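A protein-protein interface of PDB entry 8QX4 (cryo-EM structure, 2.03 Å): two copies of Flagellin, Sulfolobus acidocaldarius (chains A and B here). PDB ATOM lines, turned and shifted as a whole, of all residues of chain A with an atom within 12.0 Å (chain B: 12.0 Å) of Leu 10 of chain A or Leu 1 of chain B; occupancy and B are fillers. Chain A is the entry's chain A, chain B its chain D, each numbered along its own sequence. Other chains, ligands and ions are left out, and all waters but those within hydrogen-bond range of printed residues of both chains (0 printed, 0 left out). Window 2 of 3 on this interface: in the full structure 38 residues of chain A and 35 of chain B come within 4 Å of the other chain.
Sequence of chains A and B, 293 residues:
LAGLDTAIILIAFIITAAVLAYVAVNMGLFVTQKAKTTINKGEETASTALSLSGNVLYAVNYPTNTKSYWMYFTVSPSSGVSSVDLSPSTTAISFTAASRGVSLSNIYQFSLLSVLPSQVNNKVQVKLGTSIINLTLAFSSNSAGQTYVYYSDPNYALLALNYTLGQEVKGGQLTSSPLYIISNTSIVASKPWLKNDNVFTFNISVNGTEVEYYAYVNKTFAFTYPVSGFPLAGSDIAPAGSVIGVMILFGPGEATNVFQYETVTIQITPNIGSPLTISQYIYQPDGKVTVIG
Positions printed for both chains: 2, 3, 4, 5, 6, 7, 8 and 9. Of the 10 pairs that touch across the chains among the printed residues, none has its exchanged pair printed and touching as well.
Of the 9 printed residues of chain B, 5 touch a printed residue of chain A. Hydrophobic or aromatic side chains of chain B that line the printed part of chain A: Leu 1, Leu 4, Ile 8 and Ile 9.
Leu 10 of chain A touches Leu 1 of chain B (CA to CD1, 3.6 Å). CD1 of Leu 4 of chain B touches CD1 of Leu 10 of chain A, 3.7 Å away. CD1 of Leu 1 of chain B touches CD2 of Phe 13 of chain A, 3.96 Å away. Asp 5 of chain B touches Phe 13 of chain A (CB to O, 3.6 Å). Leu 4 of chain B touches Ile 14 of chain A. CD1 of Ile 14 of chain A touches N of Asp 5 of chain B (3.9 Å). Ile 14 of chain A touches Ile 8 of chain B. CB of Ala 17 of chain A touches O of Asp 5 of chain B, at 3.4 Å. Ile 9 of chain B touches Ala 17 of chain A (CD1 to CB, 3.7 Å). Ile 8 of chain B touches Ala 18 of chain A (CG2 to N, 3.98 Å).
No residue of chain B comes within 4 Å of Ala 7 of chain A. No residue of chain B comes within 4 Å of Ile 9 of chain A. Leu 10 of chain A touches two residues of chain B. No residue of chain B comes within 4 Å of Ile 11 of chain A. Of chain B, only Leu 1 and Asp 5 come within 4 Å of Phe 13 of chain A. Ile 15 of chain A touches none of the printed residues of chain B. Printed residues of chain B within 4 Å of Ala 17 of chain A: Asp 5 (3.4 Å) and Ile 9 (3.7 Å). Of the printed residues of chain B, Ala 18 of chain A touches Ile 8 (3.98 Å). Of chain A, only Leu 10 (3.6 Å) and Phe 13 (3.96 Å) come within 4 Å of Leu 1 of chain B. No residue of chain A comes within 4 Å of Ala 2 of chain B. Of chain A, only Leu 10 and Ile 14 come within 4 Å of Leu 4 of chain B. Of the printed residues of chain A, Ile 8 of chain B touches Ile 14 (3.7 Å) and Ala 18 (3.98 Å).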
ATOM      1  N   ALA A   2      -0.307 -24.743  13.507  1.00  0.00           N
ATOM      2  CA  ALA A   2       0.235 -23.821  14.499  1.00  0.00           C
ATOM      3  C   ALA A   2      -0.698 -23.634  15.705  1.00  0.00           C
ATOM      4  O   ALA A   2      -0.264 -23.135  16.741  1.00  0.00           O
ATOM      5  CB  ALA A   2       0.586 -22.506  13.839  1.00  0.00           C
ATOM      6  N   GLY A   3      -1.972 -24.039  15.590  1.00  0.00           N
ATOM      7  CA  GLY A   3      -2.947 -23.866  16.660  1.00  0.00           C
ATOM      8  C   GLY A   3      -2.772 -24.838  17.831  1.00  0.00           C
ATOM      9  O   GLY A   3      -3.678 -24.954  18.660  1.00  0.00           O
ATOM     10  N   LEU A   4      -1.618 -25.530  17.900  1.00  0.00           N
ATOM     11  CA  LEU A   4      -1.355 -26.536  18.923  1.00  0.00           C
ATOM     12  C   LEU A   4       0.008 -26.329  19.594  1.00  0.00           C
ATOM     13  O   LEU A   4       0.070 -26.214  20.819  1.00  0.00           O
ATOM     14  CB  LEU A   4      -1.498 -27.942  18.324  1.00  0.00           C
ATOM     15  CG  LEU A   4      -2.917 -28.353  17.927  1.00  0.00           C
ATOM     16  CD1 LEU A   4      -2.892 -29.547  16.984  1.00  0.00           C
ATOM     17  CD2 LEU A   4      -3.770 -28.659  19.150  1.00  0.00           C
ATOM     18  N   ASP A   5       1.088 -26.242  18.802  1.00  0.00           N
ATOM     19  CA  ASP A   5       2.437 -26.061  19.337  1.00  0.00           C
ATOM     20  C   ASP A   5       2.541 -24.765  20.152  1.00  0.00           C
ATOM     21  O   ASP A   5       3.109 -24.769  21.249  1.00  0.00           O
ATOM     22  CB  ASP A   5       3.524 -26.271  18.271  1.00  0.00           C
ATOM     23  CG  ASP A   5       3.690 -25.148  17.256  1.00  0.00           C
ATOM     24  OD1 ASP A   5       2.696 -24.459  16.973  1.00  0.00           O
ATOM     25  OD2 ASP A   5       4.820 -24.983  16.743  1.00  0.00           O
ATOM     26  N   THR A   6       1.926 -23.682  19.645  1.00  0.00           N
ATOM     27  CA  THR A   6       1.813 -22.403  20.344  1.00  0.00           C
ATOM     28  C   THR A   6       1.078 -22.526  21.682  1.00  0.00           C
ATOM     29  O   THR A   6       1.482 -21.891  22.656  1.00  0.00           O
ATOM     30  CB  THR A   6       1.117 -21.331  19.494  1.00  0.00           C
ATOM     31  OG1 THR A   6      -0.166 -21.810  19.089  1.00  0.00           O
ATOM     32  CG2 THR A   6       1.916 -20.925  18.278  1.00  0.00           C
ATOM     33  N   ALA A   7      -0.001 -23.323  21.729  1.00  0.00           N
ATOM     34  CA  ALA A   7      -0.812 -23.507  22.928  1.00  0.00           C
ATOM     35  C   ALA A   7      -0.015 -24.193  24.043  1.00  0.00           C
ATOM     36  O   ALA A   7      -0.112 -23.793  25.205  1.00  0.00           O
ATOM     37  CB  ALA A   7      -2.084 -24.248  22.586  1.00  0.00           C
ATOM     38  N   ILE A   8       0.811 -25.181  23.679  1.00  0.00           N
ATOM     39  CA  ILE A   8       1.683 -25.896  24.604  1.00  0.00           C
ATOM     40  C   ILE A   8       2.697 -24.939  25.237  1.00  0.00           C
ATOM     41  O   ILE A   8       2.857 -24.934  26.460  1.00  0.00           O
ATOM     42  CB  ILE A   8       2.321 -27.113  23.904  1.00  0.00           C
ATOM     43  CG1 ILE A   8       1.261 -28.180  23.633  1.00  0.00           C
ATOM     44  CG2 ILE A   8       3.494 -27.681  24.698  1.00  0.00           C
ATOM     45  CD1 ILE A   8       1.696 -29.275  22.688  1.00  0.00           C
ATOM     46  N   ILE A   9       3.346 -24.100  24.418  1.00  0.00           N
ATOM     47  CA  ILE A   9       4.332 -23.143  24.909  1.00  0.00           C
ATOM     48  C   ILE A   9       3.675 -22.111  25.828  1.00  0.00           C
ATOM     49  O   ILE A   9       4.246 -21.760  26.858  1.00  0.00           O
ATOM     50  CB  ILE A   9       5.133 -22.512  23.753  1.00  0.00           C
ATOM     51  CG1 ILE A   9       5.939 -23.590  23.029  1.00  0.00           C
ATOM     52  CG2 ILE A   9       6.032 -21.381  24.248  1.00  0.00           C
ATOM     53  CD1 ILE A   9       6.267 -23.256  21.602  1.00  0.00           C
ATOM     54  N   LEU A  10       2.462 -21.663  25.479  1.00  0.00           N
ATOM     55  CA  LEU A  10       1.672 -20.782  26.326  1.00  0.00           C
ATOM     56  C   LEU A  10       1.435 -21.413  27.703  1.00  0.00           C
ATOM     57  O   LEU A  10       1.740 -20.780  28.711  1.00  0.00           O
ATOM     58  CB  LEU A  10       0.382 -20.396  25.592  1.00  0.00           C
ATOM     59  CG  LEU A  10      -0.667 -19.632  26.403  1.00  0.00           C
ATOM     60  CD1 LEU A  10      -0.106 -18.338  26.979  1.00  0.00           C
ATOM     61  CD2 LEU A  10      -1.895 -19.348  25.555  1.00  0.00           C
ATOM     62  N   ILE A  11       0.956 -22.665  27.754  1.00  0.00           N
ATOM     63  CA  ILE A  11       0.761 -23.408  28.999  1.00  0.00           C
ATOM     64  C   ILE A  11       2.037 -23.380  29.855  1.00  0.00           C
ATOM     65  O   ILE A  11       1.993 -22.995  31.025  1.00  0.00           O
ATOM     66  CB  ILE A  11       0.225 -24.829  28.700  1.00  0.00           C
ATOM     67  CG1 ILE A  11      -1.245 -24.785  28.265  1.00  0.00           C
ATOM     68  CG2 ILE A  11       0.431 -25.791  29.866  1.00  0.00           C
ATOM     69  CD1 ILE A  11      -1.736 -26.031  27.555  1.00  0.00           C
ATOM     70  N   ALA A  12       3.180 -23.725  29.251  1.00  0.00           N
ATOM     71  CA  ALA A  12       4.474 -23.780  29.922  1.00  0.00           C
ATOM     72  C   ALA A  12       4.917 -22.414  30.463  1.00  0.00           C
ATOM     73  O   ALA A  12       5.402 -22.324  31.593  1.00  0.00           O
ATOM     74  CB  ALA A  12       5.489 -24.371  28.976  1.00  0.00           C
ATOM     75  N   PHE A  13       4.743 -21.351  29.667  1.00  0.00           N
ATOM     76  CA  PHE A  13       5.141 -20.001  30.047  1.00  0.00           C
ATOM     77  C   PHE A  13       4.261 -19.459  31.177  1.00  0.00           C
ATOM     78  O   PHE A  13       4.772 -18.775  32.059  1.00  0.00           O
ATOM     79  CB  PHE A  13       5.172 -19.084  28.819  1.00  0.00           C
ATOM     80  CG  PHE A  13       6.384 -19.194  27.919  1.00  0.00           C
ATOM     81  CD1 PHE A  13       7.271 -20.265  27.997  1.00  0.00           C
ATOM     82  CD2 PHE A  13       6.628 -18.220  26.957  1.00  0.00           C
ATOM     83  CE1 PHE A  13       8.371 -20.351  27.153  1.00  0.00           C
ATOM     84  CE2 PHE A  13       7.731 -18.302  26.115  1.00  0.00           C
ATOM     85  CZ  PHE A  13       8.600 -19.368  26.214  1.00  0.00           C
ATOM     86  N   ILE A  14       2.960 -19.792  31.174  1.00  0.00           N
ATOM     87  CA  ILE A  14       2.042 -19.446  32.255  1.00  0.00           C
ATOM     88  C   ILE A  14       2.527 -20.083  33.560  1.00  0.00           C
ATOM     89  O   ILE A  14       2.703 -19.380  34.551  1.00  0.00           O
ATOM     90  CB  ILE A  14       0.583 -19.828  31.910  1.00  0.00           C
ATOM     91  CG1 ILE A  14       0.015 -19.021  30.734  1.00  0.00           C
ATOM     92  CG2 ILE A  14      -0.328 -19.792  33.134  1.00  0.00           C
ATOM     93  CD1 ILE A  14      -0.273 -17.560  31.019  1.00  0.00           C
ATOM     94  N   ILE A  15       2.776 -21.399  33.544  1.00  0.00           N
ATOM     95  CA  ILE A  15       3.250 -22.140  34.707  1.00  0.00           C
ATOM     96  C   ILE A  15       4.566 -21.543  35.220  1.00  0.00           C
ATOM     97  O   ILE A  15       4.713 -21.334  36.424  1.00  0.00           O
ATOM     98  CB  ILE A  15       3.328 -23.652  34.402  1.00  0.00           C
ATOM     99  CG1 ILE A  15       1.931 -24.247  34.205  1.00  0.00           C
ATOM    100  CG2 ILE A  15       4.103 -24.399  35.482  1.00  0.00           C
ATOM    101  CD1 ILE A  15       1.915 -25.593  33.519  1.00  0.00           C
ATOM    102  N   THR A  16       5.485 -21.198  34.306  1.00  0.00           N
ATOM    103  CA  THR A  16       6.767 -20.578  34.632  1.00  0.00           C
ATOM    104  C   THR A  16       6.578 -19.252  35.378  1.00  0.00           C
ATOM    105  O   THR A  16       7.226 -19.026  36.400  1.00  0.00           O
ATOM    106  CB  THR A  16       7.647 -20.440  33.382  1.00  0.00           C
ATOM    107  OG1 THR A  16       7.855 -21.745  32.840  1.00  0.00           O
ATOM    108  CG2 THR A  16       8.988 -19.794  33.654  1.00  0.00           C
ATOM    109  N   ALA A  17       5.682 -18.388  34.881  1.00  0.00           N
ATOM    110  CA  ALA A  17       5.350 -17.117  35.513  1.00  0.00           C
ATOM    111  C   ALA A  17       4.668 -17.321  36.871  1.00  0.00           C
ATOM    112  O   ALA A  17       4.999 -16.630  37.834  1.00  0.00           O
ATOM    113  CB  ALA A  17       4.513 -16.285  34.572  1.00  0.00           C
ATOM    114  N   ALA A  18       3.733 -18.278  36.956  1.00  0.00           N
ATOM    115  CA  ALA A  18       3.028 -18.621  38.186  1.00  0.00           C
ATOM    116  C   ALA A  18       3.993 -19.083  39.286  1.00  0.00           C
ATOM    117  O   ALA A  18       3.825 -18.710  40.446  1.00  0.00           O
ATOM    118  CB  ALA A  18       1.963 -19.649  37.884  1.00  0.00           C
ATOM    119  N   VAL A  19       5.035 -19.842  38.913  1.00  0.00           N
ATOM    120  CA  VAL A  19       6.096 -20.285  39.811  1.00  0.00           C
ATOM    121  C   VAL A  19       6.874 -19.086  40.371  1.00  0.00           C
ATOM    122  O   VAL A  19       7.091 -19.018  41.583  1.00  0.00           O
ATOM    123  CB  VAL A  19       6.988 -21.354  39.141  1.00  0.00           C
ATOM    124  CG1 VAL A  19       8.345 -21.532  39.809  1.00  0.00           C
ATOM    125  CG2 VAL A  19       6.277 -22.694  39.054  1.00  0.00           C
ATOM    126  N   LEU B   1       0.803 -14.766  23.136  1.00  0.00           N
ATOM    127  CA  LEU B   1       1.732 -15.521  24.044  1.00  0.00           C
ATOM    128  C   LEU B   1       2.154 -14.663  25.238  1.00  0.00           C
ATOM    129  O   LEU B   1       1.755 -14.956  26.360  1.00  0.00           O
ATOM    130  CB  LEU B   1       2.933 -16.052  23.250  1.00  0.00           C
ATOM    131  CG  LEU B   1       3.969 -16.855  24.043  1.00  0.00           C
ATOM    132  CD1 LEU B   1       3.343 -18.047  24.748  1.00  0.00           C
ATOM    133  CD2 LEU B   1       5.098 -17.307  23.139  1.00  0.00           C
ATOM    134  N   ALA B   2       2.925 -13.587  25.004  1.00  0.00           N
ATOM    135  CA  ALA B   2       3.526 -12.800  26.075  1.00  0.00           C
ATOM    136  C   ALA B   2       2.495 -11.948  26.828  1.00  0.00           C
ATOM    137  O   ALA B   2       2.791 -11.453  27.914  1.00  0.00           O
ATOM    138  CB  ALA B   2       4.667 -11.972  25.534  1.00  0.00           C
ATOM    139  N   GLY B   3       1.290 -11.772  26.263  1.00  0.00           N
ATOM    140  CA  GLY B   3       0.248 -10.947  26.863  1.00  0.00           C
ATOM    141  C   GLY B   3      -0.426 -11.582  28.082  1.00  0.00           C
ATOM    142  O   GLY B   3      -1.453 -11.073  28.534  1.00  0.00           O
ATOM    143  N   LEU B   4       0.157 -12.674  28.614  1.00  0.00           N
ATOM    144  CA  LEU B   4      -0.428 -13.428  29.717  1.00  0.00           C
ATOM    145  C   LEU B   4       0.585 -13.695  30.836  1.00  0.00           C
ATOM    146  O   LEU B   4       0.321 -13.342  31.984  1.00  0.00           O
ATOM    147  CB  LEU B   4      -1.078 -14.709  29.179  1.00  0.00           C
ATOM    148  CG  LEU B   4      -2.360 -14.509  28.366  1.00  0.00           C
ATOM    149  CD1 LEU B   4      -2.709 -15.759  27.578  1.00  0.00           C
ATOM    150  CD2 LEU B   4      -3.524 -14.101  29.259  1.00  0.00           C
ATOM    151  N   ASP B   5       1.754 -14.269  30.507  1.00  0.00           N
ATOM    152  CA  ASP B   5       2.782 -14.572  31.500  1.00  0.00           C
ATOM    153  C   ASP B   5       3.252 -13.299  32.218  1.00  0.00           C
ATOM    154  O   ASP B   5       3.381 -13.291  33.448  1.00  0.00           O
ATOM    155  CB  ASP B   5       3.894 -15.472  30.940  1.00  0.00           C
ATOM    156  CG  ASP B   5       4.887 -14.802  30.001  1.00  0.00           C
ATOM    157  OD1 ASP B   5       4.496 -13.839  29.322  1.00  0.00           O
ATOM    158  OD2 ASP B   5       6.050 -15.265  29.946  1.00  0.00           O
ATOM    159  N   THR B   6       3.431 -12.208  31.456  1.00  0.00           N
ATOM    160  CA  THR B   6       3.753 -10.883  31.983  1.00  0.00           C
ATOM    161  C   THR B   6       2.681 -10.361  32.946  1.00  0.00           C
ATOM    162  O   THR B   6       3.023  -9.754  33.962  1.00  0.00           O
ATOM    163  CB  THR B   6       3.972  -9.846  30.873  1.00  0.00           C
ATOM    164  OG1 THR B   6       2.813  -9.796  30.041  1.00  0.00           O
ATOM    165  CG2 THR B   6       5.194 -10.123  30.029  1.00  0.00           C
ATOM    166  N   ALA B   7       1.396 -10.577  32.625  1.00  0.00           N
ATOM    167  CA  ALA B   7       0.278 -10.109  33.436  1.00  0.00           C
ATOM    168  C   ALA B   7       0.254 -10.790  34.809  1.00  0.00           C
ATOM    169  O   ALA B   7       0.014 -10.129  35.821  1.00  0.00           O
ATOM    170  CB  ALA B   7      -1.020 -10.282  32.681  1.00  0.00           C
ATOM    171  N   ILE B   8       0.559 -12.092  34.845  1.00  0.00           N
ATOM    172  CA  ILE B   8       0.644 -12.875  36.072  1.00  0.00           C
ATOM    173  C   ILE B   8       1.749 -12.334  36.985  1.00  0.00           C
ATOM    174  O   ILE B   8       1.506 -12.114  38.173  1.00  0.00           O
ATOM    175  CB  ILE B   8       0.783 -14.375  35.739  1.00  0.00           C
ATOM    176  CG1 ILE B   8      -0.532 -14.898  35.156  1.00  0.00           C
ATOM    177  CG2 ILE B   8       1.226 -15.191  36.950  1.00  0.00           C
ATOM    178  CD1 ILE B   8      -0.436 -16.263  34.517  1.00  0.00           C
ATOM    179  N   ILE B   9       2.938 -12.073  36.424  1.00  0.00           N
ATOM    180  CA  ILE B   9       4.059 -11.548  37.196  1.00  0.00           C
ATOM    181  C   ILE B   9       3.740 -10.153  37.736  1.00  0.00           C
ATOM    182  O   ILE B   9       4.063  -9.852  38.884  1.00  0.00           O
ATOM    183  CB  ILE B   9       5.374 -11.605  36.395  1.00  0.00           C
ATOM    184  CG1 ILE B   9       5.737 -13.057  36.083  1.00  0.00           C
ATOM    185  CG2 ILE B   9       6.510 -10.894  37.129  1.00  0.00           C
ATOM    186  CD1 ILE B   9       6.603 -13.218  34.867  1.00  0.00           C
